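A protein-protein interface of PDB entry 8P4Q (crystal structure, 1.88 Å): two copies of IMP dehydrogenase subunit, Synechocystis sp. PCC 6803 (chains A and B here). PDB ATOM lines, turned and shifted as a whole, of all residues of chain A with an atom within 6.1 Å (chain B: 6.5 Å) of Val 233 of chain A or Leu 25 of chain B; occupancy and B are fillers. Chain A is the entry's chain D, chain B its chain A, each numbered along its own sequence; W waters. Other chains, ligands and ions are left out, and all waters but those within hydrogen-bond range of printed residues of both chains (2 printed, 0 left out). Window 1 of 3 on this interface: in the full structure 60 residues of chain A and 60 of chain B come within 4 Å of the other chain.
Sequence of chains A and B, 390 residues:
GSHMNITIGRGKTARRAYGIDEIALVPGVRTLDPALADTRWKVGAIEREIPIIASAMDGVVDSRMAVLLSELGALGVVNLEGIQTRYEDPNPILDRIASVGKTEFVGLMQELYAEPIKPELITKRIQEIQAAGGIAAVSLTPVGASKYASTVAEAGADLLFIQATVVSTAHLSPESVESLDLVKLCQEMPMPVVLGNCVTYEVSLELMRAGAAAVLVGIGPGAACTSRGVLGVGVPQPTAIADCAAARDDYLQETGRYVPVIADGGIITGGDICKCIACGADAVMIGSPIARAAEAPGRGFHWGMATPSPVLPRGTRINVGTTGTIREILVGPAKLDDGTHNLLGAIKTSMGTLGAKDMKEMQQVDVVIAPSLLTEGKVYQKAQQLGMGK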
ATOM      1  N   VAL A 166      34.144 -19.077   0.014  1.00  0.00           N
ATOM      2  CA  VAL A 166      33.794 -18.367  -1.213  1.00  0.00           C
ATOM      3  C   VAL A 166      34.881 -18.661  -2.238  1.00  0.00           C
ATOM      4  O   VAL A 166      36.051 -18.332  -2.017  1.00  0.00           O
ATOM      5  CB  VAL A 166      33.656 -16.849  -1.002  1.00  0.00           C
ATOM      6  CG1 VAL A 166      33.245 -16.170  -2.298  1.00  0.00           C
ATOM      7  CG2 VAL A 166      32.650 -16.541   0.103  1.00  0.00           C
ATOM      8  N   ILE A 219      26.621 -19.813   1.061  1.00  0.00           N
ATOM      9  CA  ILE A 219      27.619 -19.087   1.840  1.00  0.00           C
ATOM     10  C   ILE A 219      26.958 -18.693   3.156  1.00  0.00           C
ATOM     11  O   ILE A 219      26.139 -17.769   3.195  1.00  0.00           O
ATOM     12  CB  ILE A 219      28.157 -17.855   1.106  1.00  0.00           C
ATOM     13  CG1 ILE A 219      28.867 -18.267  -0.185  1.00  0.00           C
ATOM     14  CG2 ILE A 219      29.104 -17.074   2.011  1.00  0.00           C
ATOM     15  CD1 ILE A 219      29.167 -17.087  -1.113  1.00  0.00           C
ATOM     16  N   GLY A 220      27.264 -19.429   4.222  1.00  0.00           N
ATOM     17  CA  GLY A 220      26.893 -19.038   5.562  1.00  0.00           C
ATOM     18  C   GLY A 220      25.549 -19.482   6.126  1.00  0.00           C
ATOM     19  O   GLY A 220      25.215 -19.120   7.261  1.00  0.00           O
ATOM     20  N   SER A 227      30.143 -17.132   9.404  1.00  0.00           N
ATOM     21  CA  SER A 227      30.729 -16.248   8.398  1.00  0.00           C
ATOM     22  C   SER A 227      29.828 -15.060   8.081  1.00  0.00           C
ATOM     23  O   SER A 227      30.327 -13.967   7.785  1.00  0.00           O
ATOM     24  CB  SER A 227      31.028 -17.030   7.118  1.00  0.00           C
ATOM     25  OG  SER A 227      32.109 -17.932   7.296  1.00  0.00           O
ATOM     26  N   ARG A 228      28.505 -15.252   8.109  1.00  0.00           N
ATOM     27  CA  ARG A 228      27.606 -14.142   7.818  1.00  0.00           C
ATOM     28  C   ARG A 228      27.713 -13.048   8.871  1.00  0.00           C
ATOM     29  O   ARG A 228      27.597 -11.864   8.545  1.00  0.00           O
ATOM     30  CB  ARG A 228      26.167 -14.642   7.703  1.00  0.00           C
ATOM     31  CG  ARG A 228      25.919 -15.476   6.451  1.00  0.00           C
ATOM     32  CD  ARG A 228      24.513 -16.058   6.408  1.00  0.00           C
ATOM     33  NE  ARG A 228      24.260 -16.717   5.131  1.00  0.00           N
ATOM     34  CZ  ARG A 228      23.086 -17.202   4.749  1.00  0.00           C
ATOM     35  NH1 ARG A 228      22.016 -17.112   5.521  1.00  0.00           N
ATOM     36  NH2 ARG A 228      22.983 -17.794   3.563  1.00  0.00           N
ATOM     37  N   GLY A 229      27.930 -13.415  10.128  1.00  0.00           N
ATOM     38  CA  GLY A 229      28.137 -12.421  11.160  1.00  0.00           C
ATOM     39  C   GLY A 229      29.532 -11.829  11.148  1.00  0.00           C
ATOM     40  O   GLY A 229      29.712 -10.651  11.470  1.00  0.00           O
ATOM     41  N   LEU A 231      31.640 -11.660   8.444  1.00  0.00           N
ATOM     42  CA  LEU A 231      31.966 -11.001   7.188  1.00  0.00           C
ATOM     43  C   LEU A 231      30.815 -10.232   6.556  1.00  0.00           C
ATOM     44  O   LEU A 231      31.067  -9.394   5.684  1.00  0.00           O
ATOM     45  CB  LEU A 231      32.468 -12.032   6.171  1.00  0.00           C
ATOM     46  CG  LEU A 231      33.549 -13.004   6.642  1.00  0.00           C
ATOM     47  CD1 LEU A 231      33.834 -14.021   5.544  1.00  0.00           C
ATOM     48  CD2 LEU A 231      34.800 -12.236   7.020  1.00  0.00           C
ATOM     49  N   GLY A 232      29.570 -10.527   6.926  1.00  0.00           N
ATOM     50  CA  GLY A 232      28.428  -9.888   6.301  1.00  0.00           C
ATOM     51  C   GLY A 232      28.115 -10.374   4.907  1.00  0.00           C
ATOM     52  O   GLY A 232      27.317  -9.738   4.209  1.00  0.00           O
ATOM     53  N   VAL A 233      28.724 -11.480   4.486  1.00  0.00           N
ATOM     54  CA  VAL A 233      28.605 -12.003   3.131  1.00  0.00           C
ATOM     55  C   VAL A 233      27.606 -13.148   3.112  1.00  0.00           C
ATOM     56  O   VAL A 233      27.593 -13.996   4.015  1.00  0.00           O
ATOM     57  CB  VAL A 233      29.978 -12.467   2.608  1.00  0.00           C
ATOM     58  CG1 VAL A 233      29.842 -13.132   1.253  1.00  0.00           C
ATOM     59  CG2 VAL A 233      30.944 -11.291   2.542  1.00  0.00           C
ATOM     60  N   GLY A 234      26.766 -13.177   2.083  1.00  0.00           N
ATOM     61  CA  GLY A 234      25.863 -14.293   1.896  1.00  0.00           C
ATOM     62  C   GLY A 234      24.625 -13.959   1.093  1.00  0.00           C
ATOM     63  O   GLY A 234      24.170 -12.815   1.086  1.00  0.00           O
ATOM     64  N   VAL A 235      24.071 -14.960   0.410  1.00  0.00           N
ATOM     65  CA  VAL A 235      22.803 -14.829  -0.292  1.00  0.00           C
ATOM     66  C   VAL A 235      21.923 -15.978   0.181  1.00  0.00           C
ATOM     67  O   VAL A 235      22.321 -17.141   0.079  1.00  0.00           O
ATOM     68  CB  VAL A 235      22.972 -14.879  -1.821  1.00  0.00           C
ATOM     69  CG1 VAL A 235      21.611 -14.930  -2.508  1.00  0.00           C
ATOM     70  CG2 VAL A 235      23.777 -13.683  -2.304  1.00  0.00           C
ATOM     71  N   ILE B  23      20.360  -6.447   5.205  1.00  0.00           N
ATOM     72  CA  ILE B  23      21.137  -6.531   3.977  1.00  0.00           C
ATOM     73  C   ILE B  23      22.274  -7.537   4.139  1.00  0.00           C
ATOM     74  O   ILE B  23      22.629  -7.954   5.242  1.00  0.00           O
ATOM     75  CB  ILE B  23      21.689  -5.165   3.538  1.00  0.00           C
ATOM     76  CG1 ILE B  23      22.726  -4.649   4.545  1.00  0.00           C
ATOM     77  CG2 ILE B  23      20.558  -4.135   3.403  1.00  0.00           C
ATOM     78  CD1 ILE B  23      23.464  -3.398   4.083  1.00  0.00           C
ATOM     79  N   ALA B  24      22.845  -7.920   2.999  1.00  0.00           N
ATOM     80  CA  ALA B  24      23.977  -8.832   2.951  1.00  0.00           C
ATOM     81  C   ALA B  24      24.782  -8.538   1.695  1.00  0.00           C
ATOM     82  O   ALA B  24      24.275  -7.951   0.737  1.00  0.00           O
ATOM     83  CB  ALA B  24      23.532 -10.299   2.953  1.00  0.00           C
ATOM     84  N   LEU B  25      26.038  -8.975   1.697  1.00  0.00           N
ATOM     85  CA  LEU B  25      26.963  -8.697   0.607  1.00  0.00           C
ATOM     86  C   LEU B  25      27.133  -9.924  -0.286  1.00  0.00           C
ATOM     87  O   LEU B  25      27.194 -11.060   0.197  1.00  0.00           O
ATOM     88  CB  LEU B  25      28.317  -8.252   1.161  1.00  0.00           C
ATOM     89  CG  LEU B  25      28.224  -7.197   2.268  1.00  0.00           C
ATOM     90  CD1 LEU B  25      29.602  -6.747   2.737  1.00  0.00           C
ATOM     91  CD2 LEU B  25      27.414  -5.997   1.780  1.00  0.00           C
ATOM     92  N   VAL B  26      27.232  -9.680  -1.582  1.00  0.00           N
ATOM     93  CA  VAL B  26      27.253 -10.724  -2.603  1.00  0.00           C
ATOM     94  C   VAL B  26      28.658 -10.798  -3.185  1.00  0.00           C
ATOM     95  O   VAL B  26      29.221  -9.760  -3.549  1.00  0.00           O
ATOM     96  CB  VAL B  26      26.226 -10.449  -3.716  1.00  0.00           C
ATOM     97  CG1 VAL B  26      26.186 -11.602  -4.709  1.00  0.00           C
ATOM     98  CG2 VAL B  26      24.851 -10.195  -3.113  1.00  0.00           C
ATOM     99  N   PRO B  27      29.246 -11.985  -3.303  1.00  0.00           N
ATOM    100  CA  PRO B  27      30.534 -12.097  -3.997  1.00  0.00           C
ATOM    101  C   PRO B  27      30.463 -11.519  -5.402  1.00  0.00           C
ATOM    102  O   PRO B  27      29.410 -11.501  -6.042  1.00  0.00           O
ATOM    103  CB  PRO B  27      30.798 -13.604  -4.028  1.00  0.00           C
ATOM    104  CG  PRO B  27      30.026 -14.158  -2.863  1.00  0.00           C
ATOM    105  CD  PRO B  27      28.787 -13.275  -2.757  1.00  0.00           C
ATOM    106  N   GLY B 271      31.118  -8.072  10.528  1.00  0.00           N
ATOM    107  CA  GLY B 271      30.155  -8.122   9.442  1.00  0.00           C
ATOM    108  C   GLY B 271      29.320  -6.861   9.348  1.00  0.00           C
ATOM    109  O   GLY B 271      29.014  -6.387   8.250  1.00  0.00           O
ATOM    110  N   CYS B 274      31.449  -4.264   7.595  1.00  0.00           N
ATOM    111  CA  CYS B 274      31.552  -4.469   6.153  1.00  0.00           C
ATOM    112  C   CYS B 274      30.282  -4.029   5.439  1.00  0.00           C
ATOM    113  O   CYS B 274      30.339  -3.430   4.357  1.00  0.00           O
ATOM    114  CB  CYS B 274      31.857  -5.937   5.862  1.00  0.00           C
ATOM    115  SG  CYS B 274      33.446  -6.477   6.518  1.00  0.00           S
ATOM    116  N   LYS B 275      29.124  -4.320   6.029  1.00  0.00           N
ATOM    117  CA  LYS B 275      27.870  -3.861   5.447  1.00  0.00           C
ATOM    118  C   LYS B 275      27.832  -2.343   5.347  1.00  0.00           C
ATOM    119  O   LYS B 275      27.351  -1.792   4.348  1.00  0.00           O
ATOM    120  CB  LYS B 275      26.699  -4.379   6.274  1.00  0.00           C
ATOM    121  CG  LYS B 275      26.453  -5.878   6.160  1.00  0.00           C
ATOM    122  CD  LYS B 275      25.278  -6.283   7.041  1.00  0.00           C
ATOM    123  CE  LYS B 275      25.255  -7.769   7.307  1.00  0.00           C
ATOM    124  NZ  LYS B 275      24.179  -8.121   8.278  1.00  0.00           N
ATOM    125  N   CYS B 276      28.321  -1.645   6.374  1.00  0.00           N
ATOM    126  CA  CYS B 276      28.308  -0.185   6.336  1.00  0.00           C
ATOM    127  C   CYS B 276      29.252   0.349   5.263  1.00  0.00           C
ATOM    128  O   CYS B 276      28.937   1.325   4.572  1.00  0.00           O
ATOM    129  CB  CYS B 276      28.665   0.375   7.716  1.00  0.00           C
ATOM    130  SG  CYS B 276      27.357   0.159   8.974  1.00  0.00           S
ATOM    131  N   ALA B 278      30.098  -1.247   2.507  1.00  0.00           N
ATOM    132  CA  ALA B 278      29.499  -1.573   1.218  1.00  0.00           C
ATOM    133  C   ALA B 278      28.451  -0.549   0.808  1.00  0.00           C
ATOM    134  O   ALA B 278      28.231  -0.331  -0.390  1.00  0.00           O
ATOM    135  CB  ALA B 278      28.880  -2.970   1.266  1.00  0.00           C
ATOM    136  N   CYS B 279      27.790   0.082   1.774  1.00  0.00           N
ATOM    137  CA  CYS B 279      26.780   1.089   1.483  1.00  0.00           C
ATOM    138  C   CYS B 279      27.364   2.482   1.301  1.00  0.00           C
ATOM    139  O   CYS B 279      26.607   3.417   1.023  1.00  0.00           O
ATOM    140  CB  CYS B 279      25.723   1.112   2.585  1.00  0.00           C
ATOM    141  SG  CYS B 279      24.703  -0.370   2.625  1.00  0.00           S
ATOM    142  N   SER B 350      36.628 -10.270   4.690  1.00  0.00           N
ATOM    143  CA  SER B 350      35.416 -10.022   3.915  1.00  0.00           C
ATOM    144  C   SER B 350      35.748  -9.425   2.551  1.00  0.00           C
ATOM    145  O   SER B 350      35.286  -9.918   1.515  1.00  0.00           O
ATOM    146  CB  SER B 350      34.479  -9.099   4.694  1.00  0.00           C
ATOM    147  OG  SER B 350      33.300  -8.847   3.955  1.00  0.00           O
ATOM    148  N   MET B 351      36.560  -8.363   2.532  1.00  0.00           N
ATOM    149  CA  MET B 351      36.996  -7.788   1.263  1.00  0.00           C
ATOM    150  C   MET B 351      37.601  -8.861   0.368  1.00  0.00           C
ATOM    151  O   MET B 351      37.402  -8.853  -0.851  1.00  0.00           O
ATOM    152  CB  MET B 351      38.003  -6.663   1.513  1.00  0.00           C
ATOM    153  CG  MET B 351      37.384  -5.412   2.126  1.00  0.00           C
ATOM    154  SD  MET B 351      38.595  -4.213   2.714  1.00  0.00           S
ATOM    155  CE  MET B 351      39.303  -3.582   1.193  1.00  0.00           C
ATOM    156  N   THR B 353      36.825 -12.148   0.261  1.00  0.00           N
ATOM    157  CA  THR B 353      35.783 -12.991  -0.320  1.00  0.00           C
ATOM    158  C   THR B 353      35.018 -12.256  -1.414  1.00  0.00           C
ATOM    159  O   THR B 353      34.433 -12.890  -2.299  1.00  0.00           O
ATOM    160  CB  THR B 353      34.795 -13.473   0.747  1.00  0.00           C
ATOM    161  OG1 THR B 353      34.143 -12.348   1.345  1.00  0.00           O
ATOM    162  CG2 THR B 353      35.497 -14.296   1.817  1.00  0.00           C
ATOM    163  N   LEU B 354      34.987 -10.929  -1.355  1.00  0.00           N
ATOM    164  CA  LEU B 354      34.233 -10.113  -2.292  1.00  0.00           C
ATOM    165  C   LEU B 354      35.088  -9.597  -3.444  1.00  0.00           C
ATOM    166  O   LEU B 354      34.542  -9.057  -4.412  1.00  0.00           O
ATOM    167  CB  LEU B 354      33.603  -8.931  -1.545  1.00  0.00           C
ATOM    168  CG  LEU B 354      32.628  -9.312  -0.427  1.00  0.00           C
ATOM    169  CD1 LEU B 354      32.369  -8.142   0.506  1.00  0.00           C
ATOM    170  CD2 LEU B 354      31.322  -9.820  -1.040  1.00  0.00           C
ATOM    171  N   MET B 362      35.318  -1.763  -1.990  1.00  0.00           N
ATOM    172  CA  MET B 362      34.363  -2.350  -1.057  1.00  0.00           C
ATOM    173  C   MET B 362      33.024  -1.636  -1.131  1.00  0.00           C
ATOM    174  O   MET B 362      31.969  -2.263  -0.980  1.00  0.00           O
ATOM    175  CB  MET B 362      34.918  -2.314   0.367  1.00  0.00           C
ATOM    176  CG  MET B 362      34.072  -3.063   1.391  1.00  0.00           C
ATOM    177  SD  MET B 362      33.840  -4.821   1.025  1.00  0.00           S
ATOM    178  CE  MET B 362      33.355  -5.424   2.657  1.00  0.00           C
ATOM    179  N   VAL B 365      30.507  -3.137  -3.783  1.00  0.00           N
ATOM    180  CA  VAL B 365      30.053  -4.522  -3.794  1.00  0.00           C
ATOM    181  C   VAL B 365      28.529  -4.583  -3.883  1.00  0.00           C
ATOM    182  O   VAL B 365      27.808  -3.708  -3.384  1.00  0.00           O
ATOM    183  CB  VAL B 365      30.569  -5.299  -2.569  1.00  0.00           C
ATOM    184  CG1 VAL B 365      32.074  -5.254  -2.494  1.00  0.00           C
ATOM    185  CG2 VAL B 365      30.009  -4.706  -1.300  1.00  0.00           C
ATOM    186  N   ASP B 366      28.038  -5.632  -4.538  1.00  0.00           N
ATOM    187  CA  ASP B 366      26.603  -5.838  -4.689  1.00  0.00           C
ATOM    188  C   ASP B 366      25.969  -6.222  -3.358  1.00  0.00           C
ATOM    189  O   ASP B 366      26.560  -6.945  -2.553  1.00  0.00           O
ATOM    190  CB  ASP B 366      26.333  -6.930  -5.724  1.00  0.00           C
ATOM    191  CG  ASP B 366      26.784  -6.536  -7.123  1.00  0.00           C
ATOM    192  OD1 ASP B 366      26.600  -5.360  -7.495  1.00  0.00           O
ATOM    193  OD2 ASP B 366      27.319  -7.407  -7.846  1.00  0.00           O
ATOM    194  N   VAL B 367      24.745  -5.754  -3.145  1.00  0.00           N
ATOM    195  CA  VAL B 367      24.026  -5.959  -1.897  1.00  0.00           C
ATOM    196  C   VAL B 367      22.691  -6.615  -2.208  1.00  0.00           C
ATOM    197  O   VAL B 367      22.062  -6.315  -3.229  1.00  0.00           O
ATOM    198  CB  VAL B 367      23.811  -4.627  -1.150  1.00  0.00           C
ATOM    199  CG1 VAL B 367      22.938  -4.846   0.077  1.00  0.00           C
ATOM    200  CG2 VAL B 367      25.150  -4.007  -0.783  1.00  0.00           C
ATOM    201  N   VAL B 368      22.256  -7.506  -1.321  1.00  0.00           N
ATOM    202  CA  VAL B 368      20.921  -8.087  -1.387  1.00  0.00           C
ATOM    203  C   VAL B 368      20.153  -7.654  -0.148  1.00  0.00           C
ATOM    204  O   VAL B 368      20.731  -7.471   0.930  1.00  0.00           O
ATOM    205  CB  VAL B 368      20.934  -9.631  -1.488  1.00  0.00           C
ATOM    206  CG1 VAL B 368      21.370 -10.074  -2.878  1.00  0.00           C
ATOM    207  CG2 VAL B 368      21.819 -10.231  -0.404  1.00  0.00           C
ATOM    208  N   LEU B 373      19.329 -13.559   6.224  1.00  0.00           N
ATOM    209  CA  LEU B 373      20.760 -13.742   6.441  1.00  0.00           C
ATOM    210  C   LEU B 373      21.056 -14.111   7.887  1.00  0.00           C
ATOM    211  O   LEU B 373      21.981 -14.883   8.164  1.00  0.00           O
ATOM    212  CB  LEU B 373      21.529 -12.475   6.071  1.00  0.00           C
ATOM    213  CG  LEU B 373      23.052 -12.649   6.061  1.00  0.00           C
ATOM    214  CD1 LEU B 373      23.488 -13.295   4.733  1.00  0.00           C
ATOM    215  CD2 LEU B 373      23.787 -11.342   6.299  1.00  0.00           C
HETATM  216  O   HOH W   1      22.137 -17.382   8.556  1.00  0.00           O
HETATM  217  O   HOH W   2      26.257  -9.702   9.351  1.00  0.00           O
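The backbone NH (N) of Leu 25 of chain B lies within hydrogen-bond range of the backbone carbonyl oxygen (O) of Gly 232 of chain A, 2.9 Å away. The guanidinium group (NH1) of Arg 228 of chain A lies close to the backbone carbonyl oxygen (O) of Leu 373 of chain B, 3.5 Å away. The backbone carbonyl oxygen of Leu 25 of chain B is in hydrogen-bond range of the backbone NH of Gly 234 of chain A, 2.9 Å away. The side-chain hydroxyl (OG) of Ser 350 of chain B lies within hydrogen-bond range of the backbone carbonyl oxygen (O) of Leu 231 of chain A (2.9 Å). The backbone NH (N) of Gly 271 of chain B sits at hydrogen-bond distance from the backbone carbonyl oxygen (O) of Gly 229 of chain A (3.1 Å).
The side-chain amino group (NZ) of Lys 275 of chain B sits close to the backbone carbonyl oxygen (O) of Ile 23 of chain B (3.4 Å). O of Ser 350 of chain B sits at hydrogen-bond distance from OG1 of Thr 353 of chain B, at 2.7 Å. O of Lys 275 of chain B lies within hydrogen-bond range of SG of Cys 279 of chain B, 3.5 Å away. O of Gly 220 of chain A lies close to NE of Arg 228 of chain A. The backbone carbonyl oxygen (O) of Ala 24 of chain B is in hydrogen-bond range of the backbone NH (N) of Val 368 of chain B (2.9 Å). The backbone carbonyl oxygen of Ile 219 of chain A lies within hydrogen-bond range of the guanidinium group of Arg 228 of chain A, at 2.9 Å.
Among the printed residues, merely in contact across the chains: Val 166 of chain A with Pro 27 of chain B, Val 166 of chain A with Thr 353 of chain B, Ile 219 of chain A with Pro 27 of chain B, Leu 231 of chain A with Gly 271 of chain B, Leu 231 of chain A with Cys 274 of chain B, Gly 232 of chain A with Ala 24 of chain B, Gly 232 of chain A with Gly 271 of chain B, Gly 232 of chain A with Lys 275 of chain B, Val 233 of chain A with Leu 25 of chain B, Val 233 of chain A with Ser 350 of chain B, Val 233 of chain A with Thr 353 of chain B, Val 233 of chain A with Leu 354 of chain B, Gly 234 of chain A with Ala 24 of chain B, Gly 234 of chain A with Val 368 of chain B, Gly 234 of chain A with Leu 373 of chain B and Val 235 of chain A with Val 26 of chain B.
Of chain B, only Leu 25, Ser 350, Thr 353 and Leu 354 come within 4 Å of Val 233 of chain A. Of chain A, only Gly 232, Val 233 and Gly 234 come within 4 Å of Leu 25 of chain B. Of the printed residues of chain A, Lys 275 of chain B touches Gly 232. Met 362 of chain B touches none of the printed residues of chain A. Printed residues of chain A within 4 Å of Val 368 of chain B: Gly 234 (3.8 Å).
Printed residues of chain A that touch a printed residue of chain B: Val 166, Ile 219, Arg 228, Gly 229, Leu 231, Gly 232, Val 233, Gly 234 and Val 235. Hydrophobic or aromatic side chains of chain A within 4 Å of the printed part of chain B: Val 166, Ile 219, Leu 231, Val 233 and Val 235. Along chain A the printed residues that touch a printed residue of chain B span positions 166 to 235. Among the printed residues, 21 pairs touch across the chains. Among the printed residues, no Asp or Glu carboxylate lies within 4 Å of a Lys or Arg side-chain nitrogen of the other chain.
No position is printed for both chains.
Water W1 lies within hydrogen-bond range of O of Leu 373 of chain B and NH1 of Arg 228 of chain A. Water W2 bridges O of Arg 228 of chain A (2.7 Å) and NZ of Lys 275 of chain B (2.8 Å).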
